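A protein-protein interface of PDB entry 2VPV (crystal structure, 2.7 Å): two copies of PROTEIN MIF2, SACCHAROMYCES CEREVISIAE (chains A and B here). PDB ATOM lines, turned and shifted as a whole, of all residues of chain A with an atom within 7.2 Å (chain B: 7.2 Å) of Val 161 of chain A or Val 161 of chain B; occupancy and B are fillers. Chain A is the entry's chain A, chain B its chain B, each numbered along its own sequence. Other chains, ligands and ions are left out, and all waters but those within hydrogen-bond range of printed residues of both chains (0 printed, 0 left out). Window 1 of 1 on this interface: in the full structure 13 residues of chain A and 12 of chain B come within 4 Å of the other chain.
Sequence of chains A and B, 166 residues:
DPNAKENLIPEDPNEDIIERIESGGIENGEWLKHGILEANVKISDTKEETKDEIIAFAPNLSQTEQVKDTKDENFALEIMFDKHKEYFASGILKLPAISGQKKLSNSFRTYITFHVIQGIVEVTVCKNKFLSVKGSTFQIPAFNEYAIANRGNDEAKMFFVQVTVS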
ATOM      1  N   TYR A  87      -1.703  16.373  -5.013  1.00  0.00           N
ATOM      2  CA  TYR A  87      -0.983  15.272  -4.408  1.00  0.00           C
ATOM      3  C   TYR A  87      -0.718  14.120  -5.361  1.00  0.00           C
ATOM      4  O   TYR A  87       0.369  13.558  -5.336  1.00  0.00           O
ATOM      5  CB  TYR A  87      -1.761  14.764  -3.227  1.00  0.00           C
ATOM      6  CG  TYR A  87      -1.091  13.654  -2.475  1.00  0.00           C
ATOM      7  CD1 TYR A  87      -0.077  13.930  -1.545  1.00  0.00           C
ATOM      8  CD2 TYR A  87      -1.495  12.324  -2.650  1.00  0.00           C
ATOM      9  CE1 TYR A  87       0.528  12.929  -0.827  1.00  0.00           C
ATOM     10  CE2 TYR A  87      -0.895  11.299  -1.916  1.00  0.00           C
ATOM     11  CZ  TYR A  87       0.113  11.618  -0.997  1.00  0.00           C
ATOM     12  OH  TYR A  87       0.702  10.610  -0.252  1.00  0.00           O
ATOM     13  N   PHE A  88      -1.712  13.758  -6.180  1.00  0.00           N
ATOM     14  CA  PHE A  88      -1.635  12.579  -7.046  1.00  0.00           C
ATOM     15  C   PHE A  88      -1.353  12.975  -8.487  1.00  0.00           C
ATOM     16  O   PHE A  88      -1.808  14.017  -8.950  1.00  0.00           O
ATOM     17  CB  PHE A  88      -2.975  11.854  -7.069  1.00  0.00           C
ATOM     18  CG  PHE A  88      -3.449  11.335  -5.735  1.00  0.00           C
ATOM     19  CD1 PHE A  88      -4.312  12.093  -4.937  1.00  0.00           C
ATOM     20  CD2 PHE A  88      -3.115  10.040  -5.322  1.00  0.00           C
ATOM     21  CE1 PHE A  88      -4.811  11.585  -3.712  1.00  0.00           C
ATOM     22  CE2 PHE A  88      -3.600   9.516  -4.116  1.00  0.00           C
ATOM     23  CZ  PHE A  88      -4.449  10.295  -3.297  1.00  0.00           C
ATOM     24  N   ALA A  89      -0.632  12.132  -9.211  1.00  0.00           N
ATOM     25  CA  ALA A  89      -0.635  12.158 -10.665  1.00  0.00           C
ATOM     26  C   ALA A  89      -1.813  11.307 -11.132  1.00  0.00           C
ATOM     27  O   ALA A  89      -2.190  10.332 -10.460  1.00  0.00           O
ATOM     28  CB  ALA A  89       0.648  11.595 -11.197  1.00  0.00           C
ATOM     29  N   SER A  90      -2.390  11.656 -12.281  1.00  0.00           N
ATOM     30  CA  SER A  90      -3.496  10.882 -12.824  1.00  0.00           C
ATOM     31  C   SER A  90      -3.631  11.068 -14.317  1.00  0.00           C
ATOM     32  O   SER A  90      -2.973  11.911 -14.895  1.00  0.00           O
ATOM     33  CB  SER A  90      -4.800  11.288 -12.150  1.00  0.00           C
ATOM     34  OG  SER A  90      -5.139  12.613 -12.517  1.00  0.00           O
ATOM     35  N   GLY A  91      -4.521  10.297 -14.927  1.00  0.00           N
ATOM     36  CA  GLY A  91      -4.752  10.383 -16.367  1.00  0.00           C
ATOM     37  C   GLY A  91      -5.696   9.316 -16.877  1.00  0.00           C
ATOM     38  O   GLY A  91      -6.479   8.732 -16.115  1.00  0.00           O
ATOM     39  N   TYR A 111       2.548   3.125  -7.357  1.00  0.00           N
ATOM     40  CA  TYR A 111       1.334   2.339  -7.238  1.00  0.00           C
ATOM     41  C   TYR A 111       0.301   3.012  -8.107  1.00  0.00           C
ATOM     42  O   TYR A 111       0.188   4.237  -8.102  1.00  0.00           O
ATOM     43  CB  TYR A 111       0.816   2.326  -5.815  1.00  0.00           C
ATOM     44  CG  TYR A 111       1.795   1.872  -4.782  1.00  0.00           C
ATOM     45  CD1 TYR A 111       2.533   2.802  -4.069  1.00  0.00           C
ATOM     46  CD2 TYR A 111       1.960   0.517  -4.475  1.00  0.00           C
ATOM     47  CE1 TYR A 111       3.431   2.416  -3.107  1.00  0.00           C
ATOM     48  CE2 TYR A 111       2.884   0.112  -3.516  1.00  0.00           C
ATOM     49  CZ  TYR A 111       3.609   1.084  -2.835  1.00  0.00           C
ATOM     50  OH  TYR A 111       4.512   0.769  -1.845  1.00  0.00           O
ATOM     51  N   ILE A 112      -0.459   2.204  -8.832  1.00  0.00           N
ATOM     52  CA  ILE A 112      -1.451   2.691  -9.779  1.00  0.00           C
ATOM     53  C   ILE A 112      -2.807   2.104  -9.410  1.00  0.00           C
ATOM     54  O   ILE A 112      -2.897   0.930  -9.017  1.00  0.00           O
ATOM     55  CB  ILE A 112      -1.110   2.239 -11.199  1.00  0.00           C
ATOM     56  CG1 ILE A 112       0.305   2.671 -11.564  1.00  0.00           C
ATOM     57  CG2 ILE A 112      -2.079   2.855 -12.191  1.00  0.00           C
ATOM     58  CD1 ILE A 112       0.923   1.919 -12.749  1.00  0.00           C
ATOM     59  N   THR A 113      -3.851   2.919  -9.503  1.00  0.00           N
ATOM     60  CA  THR A 113      -5.200   2.380  -9.468  1.00  0.00           C
ATOM     61  C   THR A 113      -5.822   2.699 -10.808  1.00  0.00           C
ATOM     62  O   THR A 113      -5.706   3.827 -11.282  1.00  0.00           O
ATOM     63  CB  THR A 113      -6.062   3.000  -8.340  1.00  0.00           C
ATOM     64  OG1 THR A 113      -5.453   2.734  -7.063  1.00  0.00           O
ATOM     65  CG2 THR A 113      -7.488   2.441  -8.366  1.00  0.00           C
ATOM     66  N   PHE A 114      -6.444   1.697 -11.428  1.00  0.00           N
ATOM     67  CA  PHE A 114      -7.180   1.892 -12.666  1.00  0.00           C
ATOM     68  C   PHE A 114      -8.680   1.775 -12.456  1.00  0.00           C
ATOM     69  O   PHE A 114      -9.145   1.022 -11.595  1.00  0.00           O
ATOM     70  CB  PHE A 114      -6.784   0.848 -13.679  1.00  0.00           C
ATOM     71  CG  PHE A 114      -5.420   1.026 -14.228  1.00  0.00           C
ATOM     72  CD1 PHE A 114      -4.344   0.334 -13.671  1.00  0.00           C
ATOM     73  CD2 PHE A 114      -5.205   1.832 -15.338  1.00  0.00           C
ATOM     74  CE1 PHE A 114      -3.049   0.463 -14.198  1.00  0.00           C
ATOM     75  CE2 PHE A 114      -3.919   1.971 -15.879  1.00  0.00           C
ATOM     76  CZ  PHE A 114      -2.829   1.288 -15.303  1.00  0.00           C
ATOM     77  N   HIS A 115      -9.434   2.499 -13.272  1.00  0.00           N
ATOM     78  CA  HIS A 115     -10.869   2.439 -13.215  1.00  0.00           C
ATOM     79  C   HIS A 115     -11.414   2.380 -14.634  1.00  0.00           C
ATOM     80  O   HIS A 115     -11.228   3.315 -15.410  1.00  0.00           O
ATOM     81  CB  HIS A 115     -11.437   3.644 -12.461  1.00  0.00           C
ATOM     82  CG  HIS A 115     -12.922   3.591 -12.293  1.00  0.00           C
ATOM     83  ND1 HIS A 115     -13.537   2.745 -11.395  1.00  0.00           N
ATOM     84  CD2 HIS A 115     -13.919   4.213 -12.963  1.00  0.00           C
ATOM     85  CE1 HIS A 115     -14.848   2.874 -11.494  1.00  0.00           C
ATOM     86  NE2 HIS A 115     -15.105   3.758 -12.439  1.00  0.00           N
ATOM     87  N   THR A 137     -12.708  -1.840 -11.077  1.00  0.00           N
ATOM     88  CA  THR A 137     -11.552  -1.071 -10.623  1.00  0.00           C
ATOM     89  C   THR A 137     -10.430  -2.015 -10.198  1.00  0.00           C
ATOM     90  O   THR A 137     -10.648  -2.843  -9.318  1.00  0.00           O
ATOM     91  CB  THR A 137     -11.926  -0.263  -9.356  1.00  0.00           C
ATOM     92  OG1 THR A 137     -12.852   0.778  -9.685  1.00  0.00           O
ATOM     93  CG2 THR A 137     -10.703   0.357  -8.727  1.00  0.00           C
ATOM     94  N   GLN A 139      -5.864  -2.549  -9.250  1.00  0.00           N
ATOM     95  CA  GLN A 139      -4.665  -1.911  -8.712  1.00  0.00           C
ATOM     96  C   GLN A 139      -3.409  -2.672  -9.063  1.00  0.00           C
ATOM     97  O   GLN A 139      -3.372  -3.892  -8.992  1.00  0.00           O
ATOM     98  CB  GLN A 139      -4.739  -1.793  -7.182  1.00  0.00           C
ATOM     99  CG  GLN A 139      -5.576  -0.620  -6.698  1.00  0.00           C
ATOM    100  CD  GLN A 139      -5.415  -0.299  -5.216  1.00  0.00           C
ATOM    101  OE1 GLN A 139      -4.301  -0.133  -4.706  1.00  0.00           O
ATOM    102  NE2 GLN A 139      -6.534  -0.154  -4.532  1.00  0.00           N
ATOM    103  N   PHE A 159      -9.465   5.451 -16.344  1.00  0.00           N
ATOM    104  CA  PHE A 159      -8.956   6.521 -15.546  1.00  0.00           C
ATOM    105  C   PHE A 159      -7.988   5.864 -14.579  1.00  0.00           C
ATOM    106  O   PHE A 159      -8.242   4.752 -14.114  1.00  0.00           O
ATOM    107  CB  PHE A 159     -10.103   7.182 -14.791  1.00  0.00           C
ATOM    108  CG  PHE A 159      -9.657   8.167 -13.763  1.00  0.00           C
ATOM    109  CD1 PHE A 159      -9.150   9.415 -14.139  1.00  0.00           C
ATOM    110  CD2 PHE A 159      -9.750   7.864 -12.419  1.00  0.00           C
ATOM    111  CE1 PHE A 159      -8.739  10.340 -13.183  1.00  0.00           C
ATOM    112  CE2 PHE A 159      -9.342   8.781 -11.456  1.00  0.00           C
ATOM    113  CZ  PHE A 159      -8.830  10.020 -11.841  1.00  0.00           C
ATOM    114  N   PHE A 160      -6.866   6.521 -14.295  1.00  0.00           N
ATOM    115  CA  PHE A 160      -5.952   6.024 -13.274  1.00  0.00           C
ATOM    116  C   PHE A 160      -5.432   7.129 -12.378  1.00  0.00           C
ATOM    117  O   PHE A 160      -5.394   8.302 -12.767  1.00  0.00           O
ATOM    118  CB  PHE A 160      -4.777   5.283 -13.907  1.00  0.00           C
ATOM    119  CG  PHE A 160      -3.890   6.149 -14.745  1.00  0.00           C
ATOM    120  CD1 PHE A 160      -2.888   6.911 -14.164  1.00  0.00           C
ATOM    121  CD2 PHE A 160      -4.022   6.168 -16.119  1.00  0.00           C
ATOM    122  CE1 PHE A 160      -2.040   7.715 -14.939  1.00  0.00           C
ATOM    123  CE2 PHE A 160      -3.182   6.957 -16.902  1.00  0.00           C
ATOM    124  CZ  PHE A 160      -2.183   7.735 -16.298  1.00  0.00           C
ATOM    125  N   VAL A 161      -4.997   6.725 -11.193  1.00  0.00           N
ATOM    126  CA  VAL A 161      -4.287   7.583 -10.243  1.00  0.00           C
ATOM    127  C   VAL A 161      -2.986   6.878  -9.902  1.00  0.00           C
ATOM    128  O   VAL A 161      -2.950   5.648  -9.851  1.00  0.00           O
ATOM    129  CB  VAL A 161      -5.098   7.707  -8.940  1.00  0.00           C
ATOM    130  CG1 VAL A 161      -4.422   8.623  -7.975  1.00  0.00           C
ATOM    131  CG2 VAL A 161      -6.498   8.212  -9.239  1.00  0.00           C
ATOM    132  N   GLN A 162      -1.916   7.635  -9.688  1.00  0.00           N
ATOM    133  CA  GLN A 162      -0.662   7.015  -9.275  1.00  0.00           C
ATOM    134  C   GLN A 162       0.197   7.828  -8.323  1.00  0.00           C
ATOM    135  O   GLN A 162       0.189   9.061  -8.316  1.00  0.00           O
ATOM    136  CB  GLN A 162       0.175   6.525 -10.468  1.00  0.00           C
ATOM    137  CG  GLN A 162       0.594   7.601 -11.421  1.00  0.00           C
ATOM    138  CD  GLN A 162       1.974   7.359 -11.981  1.00  0.00           C
ATOM    139  OE1 GLN A 162       2.207   6.381 -12.681  1.00  0.00           O
ATOM    140  NE2 GLN A 162       2.907   8.263 -11.680  1.00  0.00           N
ATOM    141  N   VAL A 163       0.967   7.104  -7.533  1.00  0.00           N
ATOM    142  CA  VAL A 163       1.818   7.703  -6.548  1.00  0.00           C
ATOM    143  C   VAL A 163       3.147   6.998  -6.701  1.00  0.00           C
ATOM    144  O   VAL A 163       3.189   5.775  -6.858  1.00  0.00           O
ATOM    145  CB  VAL A 163       1.236   7.480  -5.145  1.00  0.00           C
ATOM    146  CG1 VAL A 163       2.323   7.534  -4.094  1.00  0.00           C
ATOM    147  CG2 VAL A 163       0.160   8.495  -4.861  1.00  0.00           C
ATOM    148  N   PHE B  88      -4.126   1.644  -2.230  1.00  0.00           N
ATOM    149  CA  PHE B  88      -5.114   2.711  -2.175  1.00  0.00           C
ATOM    150  C   PHE B  88      -6.474   2.226  -1.730  1.00  0.00           C
ATOM    151  O   PHE B  88      -6.841   1.071  -1.943  1.00  0.00           O
ATOM    152  CB  PHE B  88      -5.368   3.288  -3.553  1.00  0.00           C
ATOM    153  CG  PHE B  88      -4.195   3.939  -4.193  1.00  0.00           C
ATOM    154  CD1 PHE B  88      -3.459   3.271  -5.156  1.00  0.00           C
ATOM    155  CD2 PHE B  88      -3.886   5.263  -3.919  1.00  0.00           C
ATOM    156  CE1 PHE B  88      -2.415   3.908  -5.801  1.00  0.00           C
ATOM    157  CE2 PHE B  88      -2.837   5.893  -4.558  1.00  0.00           C
ATOM    158  CZ  PHE B  88      -2.107   5.216  -5.491  1.00  0.00           C
ATOM    159  N   ALA B  89      -7.254   3.145  -1.179  1.00  0.00           N
ATOM    160  CA  ALA B  89      -8.680   2.940  -0.997  1.00  0.00           C
ATOM    161  C   ALA B  89      -9.333   3.627  -2.161  1.00  0.00           C
ATOM    162  O   ALA B  89      -8.802   4.645  -2.659  1.00  0.00           O
ATOM    163  CB  ALA B  89      -9.145   3.568   0.303  1.00  0.00           C
ATOM    164  N   SER B  90     -10.473   3.095  -2.600  1.00  0.00           N
ATOM    165  CA  SER B  90     -11.242   3.737  -3.672  1.00  0.00           C
ATOM    166  C   SER B  90     -12.755   3.587  -3.451  1.00  0.00           C
ATOM    167  O   SER B  90     -13.188   2.857  -2.564  1.00  0.00           O
ATOM    168  CB  SER B  90     -10.848   3.119  -5.008  1.00  0.00           C
ATOM    169  OG  SER B  90     -11.189   1.744  -4.990  1.00  0.00           O
ATOM    170  N   GLY B  91     -13.565   4.264  -4.256  1.00  0.00           N
ATOM    171  CA  GLY B  91     -15.003   4.072  -4.153  1.00  0.00           C
ATOM    172  C   GLY B  91     -15.850   4.854  -5.132  1.00  0.00           C
ATOM    173  O   GLY B  91     -15.345   5.481  -6.070  1.00  0.00           O
ATOM    174  N   THR B 110      -6.462  12.999   4.685  1.00  0.00           N
ATOM    175  CA  THR B 110      -6.740  12.259   3.474  1.00  0.00           C
ATOM    176  C   THR B 110      -6.602  13.137   2.255  1.00  0.00           C
ATOM    177  O   THR B 110      -7.127  14.247   2.231  1.00  0.00           O
ATOM    178  CB  THR B 110      -8.144  11.674   3.543  1.00  0.00           C
ATOM    179  OG1 THR B 110      -8.118  10.552   4.427  1.00  0.00           O
ATOM    180  CG2 THR B 110      -8.609  11.194   2.190  1.00  0.00           C
ATOM    181  N   TYR B 111      -5.849  12.647   1.272  1.00  0.00           N
ATOM    182  CA  TYR B 111      -5.822  13.202  -0.064  1.00  0.00           C
ATOM    183  C   TYR B 111      -6.784  12.405  -0.926  1.00  0.00           C
ATOM    184  O   TYR B 111      -6.782  11.178  -0.889  1.00  0.00           O
ATOM    185  CB  TYR B 111      -4.412  13.118  -0.635  1.00  0.00           C
ATOM    186  CG  TYR B 111      -3.459  14.022   0.082  1.00  0.00           C
ATOM    187  CD1 TYR B 111      -2.556  13.528   1.008  1.00  0.00           C
ATOM    188  CD2 TYR B 111      -3.496  15.385  -0.131  1.00  0.00           C
ATOM    189  CE1 TYR B 111      -1.696  14.376   1.696  1.00  0.00           C
ATOM    190  CE2 TYR B 111      -2.648  16.247   0.543  1.00  0.00           C
ATOM    191  CZ  TYR B 111      -1.760  15.751   1.459  1.00  0.00           C
ATOM    192  OH  TYR B 111      -0.957  16.667   2.117  1.00  0.00           O
ATOM    193  N   ILE B 112      -7.621  13.104  -1.687  1.00  0.00           N
ATOM    194  CA  ILE B 112      -8.615  12.447  -2.517  1.00  0.00           C
ATOM    195  C   ILE B 112      -8.545  12.934  -3.951  1.00  0.00           C
ATOM    196  O   ILE B 112      -8.325  14.132  -4.202  1.00  0.00           O
ATOM    197  CB  ILE B 112     -10.038  12.707  -2.006  1.00  0.00           C
ATOM    198  CG1 ILE B 112     -10.090  12.541  -0.486  1.00  0.00           C
ATOM    199  CG2 ILE B 112     -11.056  11.797  -2.740  1.00  0.00           C
ATOM    200  CD1 ILE B 112     -11.344  13.102   0.165  1.00  0.00           C
ATOM    201  N   THR B 113      -8.728  11.998  -4.882  1.00  0.00           N
ATOM    202  CA  THR B 113      -8.968  12.344  -6.263  1.00  0.00           C
ATOM    203  C   THR B 113     -10.329  11.817  -6.656  1.00  0.00           C
ATOM    204  O   THR B 113     -10.648  10.660  -6.380  1.00  0.00           O
ATOM    205  CB  THR B 113      -7.907  11.753  -7.206  1.00  0.00           C
ATOM    206  OG1 THR B 113      -6.612  12.192  -6.796  1.00  0.00           O
ATOM    207  CG2 THR B 113      -8.140  12.234  -8.619  1.00  0.00           C
ATOM    208  N   PHE B 114     -11.111  12.685  -7.298  1.00  0.00           N
ATOM    209  CA  PHE B 114     -12.421  12.352  -7.850  1.00  0.00           C
ATOM    210  C   PHE B 114     -12.375  12.428  -9.368  1.00  0.00           C
ATOM    211  O   PHE B 114     -11.751  13.334  -9.954  1.00  0.00           O
ATOM    212  CB  PHE B 114     -13.487  13.350  -7.392  1.00  0.00           C
ATOM    213  CG  PHE B 114     -13.830  13.253  -5.941  1.00  0.00           C
ATOM    214  CD1 PHE B 114     -13.162  14.029  -5.002  1.00  0.00           C
ATOM    215  CD2 PHE B 114     -14.845  12.414  -5.518  1.00  0.00           C
ATOM    216  CE1 PHE B 114     -13.492  13.956  -3.661  1.00  0.00           C
ATOM    217  CE2 PHE B 114     -15.185  12.321  -4.166  1.00  0.00           C
ATOM    218  CZ  PHE B 114     -14.504  13.086  -3.235  1.00  0.00           C
ATOM    219  N   HIS B 115     -13.052  11.470  -9.992  1.00  0.00           N
ATOM    220  CA  HIS B 115     -13.235  11.453 -11.425  1.00  0.00           C
ATOM    221  C   HIS B 115     -14.716  11.296 -11.684  1.00  0.00           C
ATOM    222  O   HIS B 115     -15.359  10.406 -11.104  1.00  0.00           O
ATOM    223  CB  HIS B 115     -12.495  10.283 -12.033  1.00  0.00           C
ATOM    224  CG  HIS B 115     -12.591  10.225 -13.523  1.00  0.00           C
ATOM    225  ND1 HIS B 115     -12.070  11.208 -14.340  1.00  0.00           N
ATOM    226  CD2 HIS B 115     -13.120   9.292 -14.349  1.00  0.00           C
ATOM    227  CE1 HIS B 115     -12.281  10.886 -15.602  1.00  0.00           C
ATOM    228  NE2 HIS B 115     -12.921   9.729 -15.637  1.00  0.00           N
ATOM    229  N   THR B 137     -11.804  15.661 -13.707  1.00  0.00           N
ATOM    230  CA  THR B 137     -11.075  15.128 -12.559  1.00  0.00           C
ATOM    231  C   THR B 137     -10.653  16.250 -11.620  1.00  0.00           C
ATOM    232  O   THR B 137     -10.191  17.292 -12.084  1.00  0.00           O
ATOM    233  CB  THR B 137      -9.810  14.403 -13.043  1.00  0.00           C
ATOM    234  OG1 THR B 137     -10.191  13.267 -13.815  1.00  0.00           O
ATOM    235  CG2 THR B 137      -8.987  13.922 -11.905  1.00  0.00           C
ATOM    236  N   GLN B 139      -8.969  17.197  -7.355  1.00  0.00           N
ATOM    237  CA  GLN B 139      -8.339  16.663  -6.167  1.00  0.00           C
ATOM    238  C   GLN B 139      -8.666  17.488  -4.950  1.00  0.00           C
ATOM    239  O   GLN B 139      -8.813  18.697  -5.039  1.00  0.00           O
ATOM    240  CB  GLN B 139      -6.824  16.577  -6.341  1.00  0.00           C
ATOM    241  CG  GLN B 139      -6.409  15.563  -7.355  1.00  0.00           C
ATOM    242  CD  GLN B 139      -4.949  15.193  -7.266  1.00  0.00           C
ATOM    243  OE1 GLN B 139      -4.393  14.988  -6.181  1.00  0.00           O
ATOM    244  NE2 GLN B 139      -4.319  15.063  -8.414  1.00  0.00           N
ATOM    245  N   PHE B 159     -15.966   8.334  -9.259  1.00  0.00           N
ATOM    246  CA  PHE B 159     -15.039   7.373  -8.762  1.00  0.00           C
ATOM    247  C   PHE B 159     -14.007   8.192  -8.041  1.00  0.00           C
ATOM    248  O   PHE B 159     -13.674   9.291  -8.484  1.00  0.00           O
ATOM    249  CB  PHE B 159     -14.391   6.639  -9.909  1.00  0.00           C
ATOM    250  CG  PHE B 159     -13.224   5.820  -9.498  1.00  0.00           C
ATOM    251  CD1 PHE B 159     -13.405   4.653  -8.788  1.00  0.00           C
ATOM    252  CD2 PHE B 159     -11.947   6.231  -9.798  1.00  0.00           C
ATOM    253  CE1 PHE B 159     -12.317   3.878  -8.416  1.00  0.00           C
ATOM    254  CE2 PHE B 159     -10.857   5.477  -9.422  1.00  0.00           C
ATOM    255  CZ  PHE B 159     -11.038   4.292  -8.728  1.00  0.00           C
ATOM    256  N   PHE B 160     -13.509   7.685  -6.924  1.00  0.00           N
ATOM    257  CA  PHE B 160     -12.497   8.407  -6.183  1.00  0.00           C
ATOM    258  C   PHE B 160     -11.410   7.483  -5.659  1.00  0.00           C
ATOM    259  O   PHE B 160     -11.640   6.294  -5.402  1.00  0.00           O
ATOM    260  CB  PHE B 160     -13.126   9.216  -5.046  1.00  0.00           C
ATOM    261  CG  PHE B 160     -13.724   8.378  -3.972  1.00  0.00           C
ATOM    262  CD1 PHE B 160     -12.934   7.866  -2.956  1.00  0.00           C
ATOM    263  CD2 PHE B 160     -15.079   8.098  -3.970  1.00  0.00           C
ATOM    264  CE1 PHE B 160     -13.480   7.084  -1.945  1.00  0.00           C
ATOM    265  CE2 PHE B 160     -15.652   7.314  -2.968  1.00  0.00           C
ATOM    266  CZ  PHE B 160     -14.842   6.806  -1.945  1.00  0.00           C
ATOM    267  N   VAL B 161     -10.212   8.034  -5.521  1.00  0.00           N
ATOM    268  CA  VAL B 161      -9.097   7.314  -4.912  1.00  0.00           C
ATOM    269  C   VAL B 161      -8.583   8.166  -3.761  1.00  0.00           C
ATOM    270  O   VAL B 161      -8.609   9.408  -3.823  1.00  0.00           O
ATOM    271  CB  VAL B 161      -7.967   7.071  -5.923  1.00  0.00           C
ATOM    272  CG1 VAL B 161      -6.817   6.411  -5.265  1.00  0.00           C
ATOM    273  CG2 VAL B 161      -8.449   6.195  -7.022  1.00  0.00           C
ATOM    274  N   GLN B 162      -8.150   7.518  -2.689  1.00  0.00           N
ATOM    275  CA  GLN B 162      -7.674   8.290  -1.553  1.00  0.00           C
ATOM    276  C   GLN B 162      -6.538   7.627  -0.814  1.00  0.00           C
ATOM    277  O   GLN B 162      -6.370   6.409  -0.866  1.00  0.00           O
ATOM    278  CB  GLN B 162      -8.817   8.648  -0.594  1.00  0.00           C
ATOM    279  CG  GLN B 162      -9.521   7.457  -0.024  1.00  0.00           C
ATOM    280  CD  GLN B 162     -10.410   7.804   1.145  1.00  0.00           C
ATOM    281  OE1 GLN B 162     -11.533   8.271   0.968  1.00  0.00           O
ATOM    282  NE2 GLN B 162      -9.921   7.540   2.353  1.00  0.00           N
ATOM    283  N   VAL B 163      -5.751   8.462  -0.149  1.00  0.00           N
ATOM    284  CA  VAL B 163      -4.645   8.027   0.678  1.00  0.00           C
ATOM    285  C   VAL B 163      -4.821   8.747   2.000  1.00  0.00           C
ATOM    286  O   VAL B 163      -5.004   9.971   2.031  1.00  0.00           O
ATOM    287  CB  VAL B 163      -3.289   8.420   0.051  1.00  0.00           C
ATOM    288  CG1 VAL B 163      -2.243   8.616   1.128  1.00  0.00           C
ATOM    289  CG2 VAL B 163      -2.838   7.383  -0.949  1.00  0.00           C
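Of the printed residues of chain B, Tyr 111 of chain A touches Phe 88.
Val 161 of chain A touches one residue of chain B.
Ser 90 of chain B touches none of the printed residues of chain A.
Printed residues of chain A within 4 Å of Gln 139 of chain B: Tyr 87 (3.2 Å) and Phe 88 (2.8 Å).
The nearest residue of chain B that does not touch Val 161 of chain A is Thr 113 of chain B (4.3 Å).
Phe 88 of chain A touches Ile 112 of chain B, and with the chains exchanged Ile 112 of chain A touches Phe 88 of chain B.
Phe 88 of chain A touches Thr 113 of chain B, and with the chains exchanged Thr 113 of chain A touches Phe 88 of chain B.
His 115 of chain A touches Phe 159 of chain B, and with the chains exchanged Phe 159 of chain A touches His 115 of chain B.
Phe 159 of chain B touches its own counterpart, Phe 159 of chain A.
16 positions are printed for both chains.
The backbone NH (N) of Tyr 87 of chain A is in hydrogen-bond range of the side-chain amide oxygen (OE1) of Gln 139 of chain B, 3.2 Å away.
NE2 of Gln 139 of chain B sits at hydrogen-bond distance from O of Phe 88 of chain A, at 2.8 Å.
O of Phe 88 of chain B lies within hydrogen-bond range of NE2 of Gln 139 of chain A.
N of Tyr 111 of chain A is in hydrogen-bond range of O of Val 163 of chain A.
O of Val 161 of chain A is in hydrogen-bond range of N of Thr 113 of chain A, 2.9 Å away.
The backbone NH of His 115 of chain A lies within hydrogen-bond range of the backbone carbonyl oxygen of Phe 159 of chain A (2.7 Å).
The backbone NH (N) of Tyr 111 of chain B sits at hydrogen-bond distance from the backbone carbonyl oxygen (O) of Val 163 of chain B (2.9 Å).
The backbone NH (N) of Val 161 of chain B sits at hydrogen-bond distance from the backbone carbonyl oxygen (O) of Thr 113 of chain B.
O of Phe 159 of chain B is in hydrogen-bond range of N of His 115 of chain B (2.7 Å).
Printed residues of chain B that touch a printed residue of chain A: Phe 88, Tyr 111, Ile 112, Thr 113, His 115, Thr 137, Gln 139, Phe 159, Val 161 and Val 163.
Hydrophobic or aromatic side chains of chain B that line the printed part of chain A: Phe 88, Tyr 111, His 115, Phe 159, Val 161 and Val 163.
Hydrophobic or aromatic side chains of chain A that line the printed part of chain B: Tyr 87, Phe 88, Tyr 111, His 115, Phe 159, Val 161 and Val 163.
Among the printed residues, no Asp or Glu carboxylate lies within 4 Å of a Lys or Arg side-chain nitrogen of the other chain.
Val 163 of chain B touches Tyr 87 of chain A.
Phe 88 of chain A touches Phe 88 of chain B.
CE1 of Phe 88 of chain A touches N of Ile 112 of chain B, at 3.8 Å.
CD1 of Phe 88 of chain A touches OG1 of Thr 113 of chain B, 3.0 Å away.
CZ of Phe 88 of chain A touches N of Val 163 of chain B, 3.9 Å away.
Tyr 111 of chain A touches Phe 88 of chain B (O to CE1, 3.5 Å).
His 115 of chain A touches Phe 159 of chain B (ND1 to CD1, 3.2 Å).
Phe 159 of chain A touches Thr 137 of chain B (CE1 to OG1, 3.3 Å).
CD2 of Phe 159 of chain A touches CD2 of Phe 159 of chain B, at 3.8 Å.
Phe 88 of chain B touches Val 163 of chain A (CE2 to CG2, 3.98 Å).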
